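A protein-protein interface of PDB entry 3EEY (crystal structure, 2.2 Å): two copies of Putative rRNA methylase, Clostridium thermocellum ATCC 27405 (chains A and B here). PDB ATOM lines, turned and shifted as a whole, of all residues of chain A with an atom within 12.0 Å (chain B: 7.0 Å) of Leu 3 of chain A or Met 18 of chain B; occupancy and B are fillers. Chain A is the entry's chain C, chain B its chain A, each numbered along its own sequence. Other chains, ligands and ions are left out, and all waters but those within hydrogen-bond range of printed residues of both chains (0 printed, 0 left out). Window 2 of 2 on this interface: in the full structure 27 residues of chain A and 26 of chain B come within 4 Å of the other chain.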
ATOM      1  N   LEU A   3     -18.376   9.213  30.623  1.00  0.00           N
ATOM      2  CA  LEU A   3     -17.737  10.412  29.995  1.00  0.00           C
ATOM      3  C   LEU A   3     -16.982  10.085  28.700  1.00  0.00           C
ATOM      4  O   LEU A   3     -16.039   9.289  28.700  1.00  0.00           O
ATOM      5  CB  LEU A   3     -16.798  11.116  30.981  1.00  0.00           C
ATOM      6  CG  LEU A   3     -16.054  12.346  30.447  1.00  0.00           C
ATOM      7  CD1 LEU A   3     -16.977  13.561  30.344  1.00  0.00           C
ATOM      8  CD2 LEU A   3     -14.858  12.654  31.320  1.00  0.00           C
ATOM      9  N   THR A   4     -17.398  10.735  27.615  1.00  0.00           N
ATOM     10  CA  THR A   4     -16.865  10.494  26.278  1.00  0.00           C
ATOM     11  C   THR A   4     -16.502  11.830  25.617  1.00  0.00           C
ATOM     12  O   THR A   4     -17.207  12.829  25.791  1.00  0.00           O
ATOM     13  CB  THR A   4     -17.902   9.732  25.404  1.00  0.00           C
ATOM     14  OG1 THR A   4     -18.558   8.728  26.191  1.00  0.00           O
ATOM     15  CG2 THR A   4     -17.241   9.067  24.197  1.00  0.00           C
ATOM     16  N   ILE A   5     -15.388  11.840  24.884  1.00  0.00           N
ATOM     17  CA  ILE A   5     -15.007  12.974  24.034  1.00  0.00           C
ATOM     18  C   ILE A   5     -16.040  13.134  22.914  1.00  0.00           C
ATOM     19  O   ILE A   5     -16.332  12.192  22.169  1.00  0.00           O
ATOM     20  CB  ILE A   5     -13.551  12.825  23.475  1.00  0.00           C
ATOM     21  CG1 ILE A   5     -12.528  13.080  24.586  1.00  0.00           C
ATOM     22  CG2 ILE A   5     -13.277  13.777  22.296  1.00  0.00           C
ATOM     23  CD1 ILE A   5     -11.114  12.649  24.254  1.00  0.00           C
ATOM     24  N   LYS A   6     -16.609  14.333  22.831  1.00  0.00           N
ATOM     25  CA  LYS A   6     -17.648  14.623  21.860  1.00  0.00           C
ATOM     26  C   LYS A   6     -17.056  14.902  20.499  1.00  0.00           C
ATOM     27  O   LYS A   6     -15.903  15.321  20.401  1.00  0.00           O
ATOM     28  CB  LYS A   6     -18.491  15.802  22.324  1.00  0.00           C
ATOM     29  CG  LYS A   6     -19.245  15.520  23.602  1.00  0.00           C
ATOM     30  CD  LYS A   6     -20.048  16.717  24.044  1.00  0.00           C
ATOM     31  CE  LYS A   6     -20.509  16.548  25.472  1.00  0.00           C
ATOM     32  NZ  LYS A   6     -21.142  17.782  25.974  1.00  0.00           N
ATOM     33  N   ASN A   7     -17.850  14.657  19.453  1.00  0.00           N
ATOM     34  CA  ASN A   7     -17.512  15.061  18.097  1.00  0.00           C
ATOM     35  C   ASN A   7     -17.459  16.594  17.970  1.00  0.00           C
ATOM     36  O   ASN A   7     -17.813  17.307  18.908  1.00  0.00           O
ATOM     37  CB  ASN A   7     -18.460  14.405  17.071  1.00  0.00           C
ATOM     38  CG  ASN A   7     -19.919  14.865  17.189  1.00  0.00           C
ATOM     39  OD1 ASN A   7     -20.283  15.677  18.032  1.00  0.00           O
ATOM     40  ND2 ASN A   7     -20.759  14.329  16.319  1.00  0.00           N
ATOM     41  N   GLY A  10     -20.702  18.477  18.756  1.00  0.00           N
ATOM     42  CA  GLY A  10     -20.952  18.508  20.191  1.00  0.00           C
ATOM     43  C   GLY A  10     -20.034  19.449  20.943  1.00  0.00           C
ATOM     44  O   GLY A  10     -20.453  20.119  21.877  1.00  0.00           O
ATOM     45  N   GLN A  11     -18.778  19.494  20.529  1.00  0.00           N
ATOM     46  CA  GLN A  11     -17.784  20.340  21.169  1.00  0.00           C
ATOM     47  C   GLN A  11     -18.011  21.830  20.936  1.00  0.00           C
ATOM     48  O   GLN A  11     -17.728  22.636  21.819  1.00  0.00           O
ATOM     49  CB  GLN A  11     -16.383  19.943  20.716  1.00  0.00           C
ATOM     50  CG  GLN A  11     -15.876  18.654  21.337  1.00  0.00           C
ATOM     51  CD  GLN A  11     -14.401  18.441  21.102  1.00  0.00           C
ATOM     52  OE1 GLN A  11     -13.584  19.296  21.438  1.00  0.00           O
ATOM     53  NE2 GLN A  11     -14.051  17.297  20.526  1.00  0.00           N
ATOM     54  N   ASP A  14     -20.294  23.003  23.543  1.00  0.00           N
ATOM     55  CA  ASP A  14     -19.545  23.085  24.807  1.00  0.00           C
ATOM     56  C   ASP A  14     -18.677  24.331  24.925  1.00  0.00           C
ATOM     57  O   ASP A  14     -18.621  24.947  25.990  1.00  0.00           O
ATOM     58  CB  ASP A  14     -18.678  21.840  25.006  1.00  0.00           C
ATOM     59  CG  ASP A  14     -19.487  20.611  25.377  1.00  0.00           C
ATOM     60  OD1 ASP A  14     -20.710  20.737  25.609  1.00  0.00           O
ATOM     61  OD2 ASP A  14     -18.889  19.517  25.442  1.00  0.00           O
ATOM     62  N   TYR A  15     -17.993  24.684  23.836  1.00  0.00           N
ATOM     63  CA  TYR A  15     -17.184  25.910  23.765  1.00  0.00           C
ATOM     64  C   TYR A  15     -18.035  27.173  23.830  1.00  0.00           C
ATOM     65  O   TYR A  15     -17.626  28.166  24.420  1.00  0.00           O
ATOM     66  CB  TYR A  15     -16.342  25.946  22.486  1.00  0.00           C
ATOM     67  CG  TYR A  15     -15.001  25.251  22.577  1.00  0.00           C
ATOM     68  CD1 TYR A  15     -14.808  23.997  22.009  1.00  0.00           C
ATOM     69  CD2 TYR A  15     -13.915  25.863  23.207  1.00  0.00           C
ATOM     70  CE1 TYR A  15     -13.586  23.359  22.075  1.00  0.00           C
ATOM     71  CE2 TYR A  15     -12.680  25.229  23.280  1.00  0.00           C
ATOM     72  CZ  TYR A  15     -12.523  23.977  22.708  1.00  0.00           C
ATOM     73  OH  TYR A  15     -11.302  23.338  22.757  1.00  0.00           O
ATOM     74  N   LYS A  17     -21.112  27.355  25.322  1.00  0.00           N
ATOM     75  CA  LYS A  17     -21.572  27.378  26.724  1.00  0.00           C
ATOM     76  C   LYS A  17     -20.562  27.977  27.710  1.00  0.00           C
ATOM     77  O   LYS A  17     -20.954  28.633  28.669  1.00  0.00           O
ATOM     78  CB  LYS A  17     -21.939  25.972  27.183  1.00  0.00           C
ATOM     79  CG  LYS A  17     -23.375  25.560  26.902  1.00  0.00           C
ATOM     80  CD  LYS A  17     -23.511  24.047  26.718  1.00  0.00           C
ATOM     81  CE  LYS A  17     -22.812  23.229  27.805  1.00  0.00           C
ATOM     82  NZ  LYS A  17     -23.757  22.510  28.702  1.00  0.00           N
ATOM     83  N   MET A  18     -19.275  27.739  27.466  1.00  0.00           N
ATOM     84  CA  MET A  18     -18.200  28.297  28.282  1.00  0.00           C
ATOM     85  C   MET A  18     -18.115  29.805  28.171  1.00  0.00           C
ATOM     86  O   MET A  18     -17.815  30.480  29.150  1.00  0.00           O
ATOM     87  CB  MET A  18     -16.855  27.726  27.849  1.00  0.00           C
ATOM     88  CG  MET A  18     -16.375  26.517  28.638  1.00  0.00           C
ATOM     89  SD  MET A  18     -15.129  25.573  27.728  1.00  0.00           S
ATOM     90  CE  MET A  18     -14.043  26.853  27.093  1.00  0.00           C
ATOM     91  N   THR A 170      -9.381  21.263  15.916  1.00  0.00           N
ATOM     92  CA  THR A 170      -9.587  19.991  16.589  1.00  0.00           C
ATOM     93  C   THR A 170     -10.001  18.959  15.542  1.00  0.00           C
ATOM     94  O   THR A 170     -10.910  19.201  14.773  1.00  0.00           O
ATOM     95  CB  THR A 170     -10.672  20.115  17.677  1.00  0.00           C
ATOM     96  OG1 THR A 170     -10.259  21.083  18.656  1.00  0.00           O
ATOM     97  CG2 THR A 170     -10.909  18.793  18.360  1.00  0.00           C
ATOM     98  N   PHE A 172     -10.163  14.582  14.505  1.00  0.00           N
ATOM     99  CA  PHE A 172     -10.145  13.162  14.859  1.00  0.00           C
ATOM    100  C   PHE A 172      -9.433  12.364  13.783  1.00  0.00           C
ATOM    101  O   PHE A 172     -10.017  12.021  12.754  1.00  0.00           O
ATOM    102  CB  PHE A 172     -11.562  12.657  15.100  1.00  0.00           C
ATOM    103  CG  PHE A 172     -12.267  13.410  16.190  1.00  0.00           C
ATOM    104  CD1 PHE A 172     -12.114  13.027  17.515  1.00  0.00           C
ATOM    105  CD2 PHE A 172     -13.047  14.535  15.897  1.00  0.00           C
ATOM    106  CE1 PHE A 172     -12.740  13.735  18.536  1.00  0.00           C
ATOM    107  CE2 PHE A 172     -13.677  15.248  16.910  1.00  0.00           C
ATOM    108  CZ  PHE A 172     -13.531  14.848  18.230  1.00  0.00           C
ATOM    109  N   HIS B  13      -3.680  18.909  31.041  1.00  0.00           N
ATOM    110  CA  HIS B  13      -4.081  18.900  32.446  1.00  0.00           C
ATOM    111  C   HIS B  13      -5.599  18.943  32.637  1.00  0.00           C
ATOM    112  O   HIS B  13      -6.137  18.238  33.493  1.00  0.00           O
ATOM    113  CB  HIS B  13      -3.428  20.071  33.170  1.00  0.00           C
ATOM    114  CG  HIS B  13      -1.969  19.878  33.436  1.00  0.00           C
ATOM    115  ND1 HIS B  13      -1.412  20.056  34.683  1.00  0.00           N
ATOM    116  CD2 HIS B  13      -0.950  19.526  32.618  1.00  0.00           C
ATOM    117  CE1 HIS B  13      -0.115  19.825  34.621  1.00  0.00           C
ATOM    118  NE2 HIS B  13       0.189  19.497  33.380  1.00  0.00           N
ATOM    119  N   ASP B  14      -6.280  19.769  31.837  1.00  0.00           N
ATOM    120  CA  ASP B  14      -7.743  19.862  31.844  1.00  0.00           C
ATOM    121  C   ASP B  14      -8.431  18.549  31.465  1.00  0.00           C
ATOM    122  O   ASP B  14      -9.428  18.175  32.086  1.00  0.00           O
ATOM    123  CB  ASP B  14      -8.230  20.986  30.920  1.00  0.00           C
ATOM    124  CG  ASP B  14      -8.029  22.377  31.517  1.00  0.00           C
ATOM    125  OD1 ASP B  14      -7.540  22.500  32.658  1.00  0.00           O
ATOM    126  OD2 ASP B  14      -8.380  23.360  30.836  1.00  0.00           O
ATOM    127  N   TYR B  15      -7.894  17.873  30.447  1.00  0.00           N
ATOM    128  CA  TYR B  15      -8.372  16.555  30.030  1.00  0.00           C
ATOM    129  C   TYR B  15      -8.129  15.478  31.079  1.00  0.00           C
ATOM    130  O   TYR B  15      -8.956  14.587  31.248  1.00  0.00           O
ATOM    131  CB  TYR B  15      -7.739  16.137  28.702  1.00  0.00           C
ATOM    132  CG  TYR B  15      -8.476  16.651  27.487  1.00  0.00           C
ATOM    133  CD1 TYR B  15      -8.004  17.754  26.773  1.00  0.00           C
ATOM    134  CD2 TYR B  15      -9.647  16.034  27.047  1.00  0.00           C
ATOM    135  CE1 TYR B  15      -8.684  18.238  25.656  1.00  0.00           C
ATOM    136  CE2 TYR B  15     -10.330  16.504  25.923  1.00  0.00           C
ATOM    137  CZ  TYR B  15      -9.845  17.605  25.232  1.00  0.00           C
ATOM    138  OH  TYR B  15     -10.514  18.085  24.125  1.00  0.00           O
ATOM    139  N   ILE B  16      -7.002  15.571  31.780  1.00  0.00           N
ATOM    140  CA  ILE B  16      -6.659  14.612  32.827  1.00  0.00           C
ATOM    141  C   ILE B  16      -7.578  14.787  34.047  1.00  0.00           C
ATOM    142  O   ILE B  16      -8.072  13.800  34.589  1.00  0.00           O
ATOM    143  CB  ILE B  16      -5.128  14.658  33.203  1.00  0.00           C
ATOM    144  CG1 ILE B  16      -4.239  14.139  32.059  1.00  0.00           C
ATOM    145  CG2 ILE B  16      -4.840  13.877  34.457  1.00  0.00           C
ATOM    146  CD1 ILE B  16      -4.437  12.683  31.647  1.00  0.00           C
ATOM    147  N   LYS B  17      -7.821  16.038  34.444  1.00  0.00           N
ATOM    148  CA  LYS B  17      -8.770  16.376  35.518  1.00  0.00           C
ATOM    149  C   LYS B  17     -10.193  15.837  35.279  1.00  0.00           C
ATOM    150  O   LYS B  17     -10.858  15.431  36.229  1.00  0.00           O
ATOM    151  CB  LYS B  17      -8.828  17.895  35.727  1.00  0.00           C
ATOM    152  CG  LYS B  17      -7.834  18.462  36.730  1.00  0.00           C
ATOM    153  CD  LYS B  17      -7.419  19.891  36.381  1.00  0.00           C
ATOM    154  CE  LYS B  17      -8.599  20.826  36.105  1.00  0.00           C
ATOM    155  NZ  LYS B  17      -8.779  21.866  37.155  1.00  0.00           N
ATOM    156  N   MET B  18     -10.637  15.835  34.016  1.00  0.00           N
ATOM    157  CA  MET B  18     -11.934  15.263  33.594  1.00  0.00           C
ATOM    158  C   MET B  18     -12.064  13.774  33.888  1.00  0.00           C
ATOM    159  O   MET B  18     -13.148  13.281  34.182  1.00  0.00           O
ATOM    160  CB  MET B  18     -12.137  15.423  32.081  1.00  0.00           C
ATOM    161  CG  MET B  18     -12.697  16.750  31.572  1.00  0.00           C
ATOM    162  SD  MET B  18     -12.619  16.818  29.751  1.00  0.00           S
ATOM    163  CE  MET B  18     -14.016  15.797  29.280  1.00  0.00           C
ATOM    164  N   PHE B  19     -10.953  13.056  33.790  1.00  0.00           N
ATOM    165  CA  PHE B  19     -10.978  11.599  33.775  1.00  0.00           C
ATOM    166  C   PHE B  19     -10.478  10.964  35.066  1.00  0.00           C
ATOM    167  O   PHE B  19     -10.947   9.901  35.457  1.00  0.00           O
ATOM    168  CB  PHE B  19     -10.141  11.088  32.603  1.00  0.00           C
ATOM    169  CG  PHE B  19     -10.844  11.141  31.281  1.00  0.00           C
ATOM    170  CD1 PHE B  19     -11.419   9.993  30.752  1.00  0.00           C
ATOM    171  CD2 PHE B  19     -10.917  12.320  30.547  1.00  0.00           C
ATOM    172  CE1 PHE B  19     -12.069  10.019  29.525  1.00  0.00           C
ATOM    173  CE2 PHE B  19     -11.567  12.359  29.319  1.00  0.00           C
ATOM    174  CZ  PHE B  19     -12.146  11.203  28.807  1.00  0.00           C
ATOM    175  N   VAL B  20      -9.521  11.609  35.721  1.00  0.00           N
ATOM    176  CA  VAL B  20      -8.879  11.032  36.894  1.00  0.00           C
ATOM    177  C   VAL B  20      -9.617  11.411  38.172  1.00  0.00           C
ATOM    178  O   VAL B  20      -9.824  12.594  38.451  1.00  0.00           O
ATOM    179  CB  VAL B  20      -7.383  11.449  36.982  1.00  0.00           C
ATOM    180  CG1 VAL B  20      -6.728  10.952  38.262  1.00  0.00           C
ATOM    181  CG2 VAL B  20      -6.640  10.926  35.790  1.00  0.00           C
ATOM    182  N   LYS B  21     -10.038  10.396  38.922  1.00  0.00           N
ATOM    183  CA  LYS B  21     -10.595  10.597  40.257  1.00  0.00           C
ATOM    184  C   LYS B  21      -9.667   9.993  41.313  1.00  0.00           C
ATOM    185  O   LYS B  21      -8.635   9.395  40.980  1.00  0.00           O
ATOM    186  CB  LYS B  21     -12.031  10.049  40.363  1.00  0.00           C
ATOM    187  CG  LYS B  21     -12.195   8.543  40.166  1.00  0.00           C
ATOM    188  CD  LYS B  21     -13.631   8.112  40.446  1.00  0.00           C
ATOM    189  CE  LYS B  21     -13.799   6.602  40.363  1.00  0.00           C
ATOM    190  NZ  LYS B  21     -15.145   6.163  40.843  1.00  0.00           N
ATOM    191  N   LEU B  43      -4.162  14.671  42.228  1.00  0.00           N
ATOM    192  CA  LEU B  43      -5.488  14.263  41.754  1.00  0.00           C
ATOM    193  C   LEU B  43      -5.912  12.918  42.306  1.00  0.00           C
ATOM    194  O   LEU B  43      -7.100  12.639  42.468  1.00  0.00           O
ATOM    195  CB  LEU B  43      -5.514  14.158  40.229  1.00  0.00           C
ATOM    196  CG  LEU B  43      -5.396  15.400  39.352  1.00  0.00           C
ATOM    197  CD1 LEU B  43      -5.587  14.953  37.937  1.00  0.00           C
ATOM    198  CD2 LEU B  43      -6.416  16.480  39.719  1.00  0.00           C
ATOM    199  N   GLY B 132     -12.749   3.825  28.918  1.00  0.00           N
ATOM    200  CA  GLY B 132     -13.058   5.157  29.417  1.00  0.00           C
ATOM    201  C   GLY B 132     -11.848   5.866  30.006  1.00  0.00           C
ATOM    202  O   GLY B 132     -11.999   6.902  30.643  1.00  0.00           O
ATOM    203  N   GLY B 133     -10.657   5.302  29.795  1.00  0.00           N
ATOM    204  CA  GLY B 133      -9.398   5.901  30.239  1.00  0.00           C
ATOM    205  C   GLY B 133      -8.782   6.774  29.164  1.00  0.00           C
ATOM    206  O   GLY B 133      -9.190   6.694  28.019  1.00  0.00           O
ATOM    207  N   ILE B 134      -7.793   7.594  29.528  1.00  0.00           N
ATOM    208  CA  ILE B 134      -7.236   8.594  28.602  1.00  0.00           C
ATOM    209  C   ILE B 134      -5.713   8.605  28.559  1.00  0.00           C
ATOM    210  O   ILE B 134      -5.058   8.388  29.562  1.00  0.00           O
ATOM    211  CB  ILE B 134      -7.818  10.024  28.885  1.00  0.00           C
ATOM    212  CG1 ILE B 134      -7.463  11.007  27.766  1.00  0.00           C
ATOM    213  CG2 ILE B 134      -7.340  10.585  30.243  1.00  0.00           C
ATOM    214  CD1 ILE B 134      -8.634  11.720  27.159  1.00  0.00           C
ATOM    215  N   GLU B 186      -8.581   8.183  23.884  1.00  0.00           N
ATOM    216  CA  GLU B 186      -9.526   7.644  24.863  1.00  0.00           C
ATOM    217  C   GLU B 186      -9.993   6.269  24.437  1.00  0.00           C
ATOM    218  O   GLU B 186     -10.464   6.104  23.318  1.00  0.00           O
ATOM    219  CB  GLU B 186     -10.753   8.548  25.008  1.00  0.00           C
ATOM    220  CG  GLU B 186     -11.644   8.135  26.174  1.00  0.00           C
ATOM    221  CD  GLU B 186     -13.012   8.786  26.179  1.00  0.00           C
ATOM    222  OE1 GLU B 186     -13.240   9.745  25.423  1.00  0.00           O
ATOM    223  OE2 GLU B 186     -13.874   8.331  26.955  1.00  0.00           O
ATOM    224  N   LYS B 187      -9.876   5.289  25.329  1.00  0.00           N
ATOM    225  CA  LYS B 187     -10.370   3.941  25.059  1.00  0.00           C
ATOM    226  C   LYS B 187     -11.884   3.911  25.180  1.00  0.00           C
ATOM    227  O   LYS B 187     -12.438   4.351  26.176  1.00  0.00           O
ATOM    228  CB  LYS B 187      -9.729   2.916  26.002  1.00  0.00           C
ATOM    229  CG  LYS B 187     -10.142   1.467  25.731  1.00  0.00           C
ATOM    230  CD  LYS B 187      -9.430   0.472  26.641  1.00  0.00           C
ATOM    231  CE  LYS B 187      -8.246  -0.152  25.944  1.00  0.00           C
ATOM    232  NZ  LYS B 187      -7.451  -1.103  26.773  1.00  0.00           N
ATOM    233  N   ILE B 188     -12.553   3.407  24.146  1.00  0.00           N
ATOM    234  CA  ILE B 188     -14.013   3.315  24.162  1.00  0.00           C
ATOM    235  C   ILE B 188     -14.520   1.871  24.122  1.00  0.00           C
ATOM    236  O   ILE B 188     -15.689   1.608  24.417  1.00  0.00           O
ATOM    237  CB  ILE B 188     -14.667   4.177  23.049  1.00  0.00           C
ATOM    238  CG1 ILE B 188     -14.200   3.746  21.651  1.00  0.00           C
ATOM    239  CG2 ILE B 188     -14.399   5.654  23.303  1.00  0.00           C
ATOM    240  CD1 ILE B 188     -14.914   4.450  20.515  1.00  0.00           C
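The side-chain carboxylate of Glu 186 of chain B lies close to the backbone carbonyl oxygen of Leu 3 of chain A, at 2.9 Å. N of Ile 5 of chain A sits at hydrogen-bond distance from OE1 of Glu 186 of chain B, 3.0 Å away.
CD2 of Leu 3 of chain A touches O of Met 18 of chain B, 3.4 Å away. Phe 19 of chain B touches Leu 3 of chain A (CE2 to CD2, 3.9 Å). Thr 4 of chain A touches Glu 186 of chain B. Ile 5 of chain A touches Ile 134 of chain B (CD1 to CD1, 3.9 Å).
Leu 3 of chain A touches just these residues of chain B: Met 18, Phe 19 and Glu 186. Of the printed residues of chain B, Thr 4 of chain A touches Glu 186 (3.8 Å). Of the printed residues of chain B, Ile 5 of chain A touches Ile 134 (3.9 Å) and Glu 186 (3.0 Å). His 13 of chain B touches none of the printed residues of chain A. No residue of chain A comes within 4 Å of Tyr 15 of chain B. Ile 16 of chain B touches none of the printed residues of chain A. No residue of chain A comes within 4 Å of Lys 17 of chain B. Of chain A, only Leu 3 comes within 4 Å of Met 18 of chain B. Of the printed residues of chain A, Phe 19 of chain B touches Leu 3 (3.9 Å). No residue of chain A comes within 4 Å of Gly 132 of chain B. No residue of chain A comes within 4 Å of Gly 133 of chain B. Printed residues of chain A within 4 Å of Ile 134 of chain B: Ile 5 (3.9 Å). Printed residues of chain A within 4 Å of Glu 186 of chain B: Leu 3 (2.9 Å), Thr 4 (3.8 Å) and Ile 5 (3.0 Å). Ile 188 of chain B touches none of the printed residues of chain A. The nearest printed residue of chain A that does not touch Glu 186 of chain B is Lys 6 of chain A (6.3 Å).
Hydrophobic or aromatic side chains of chain A within 4 Å of the printed part of chain B: Leu 3 and Ile 5. Of the 16 printed residues of chain B, 4 touch a printed residue of chain A. Hydrophobic or aromatic side chains of chain B that line the printed part of chain A: Met 18, Phe 19 and Ile 134. Among the printed residues, 6 pairs touch across the chains. Among the printed residues, no Asp or Glu carboxylate lies within 4 Å of a Lys or Arg side-chain nitrogen of the other chain.
Positions printed for both chains: 14, 15, 17 and 18.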
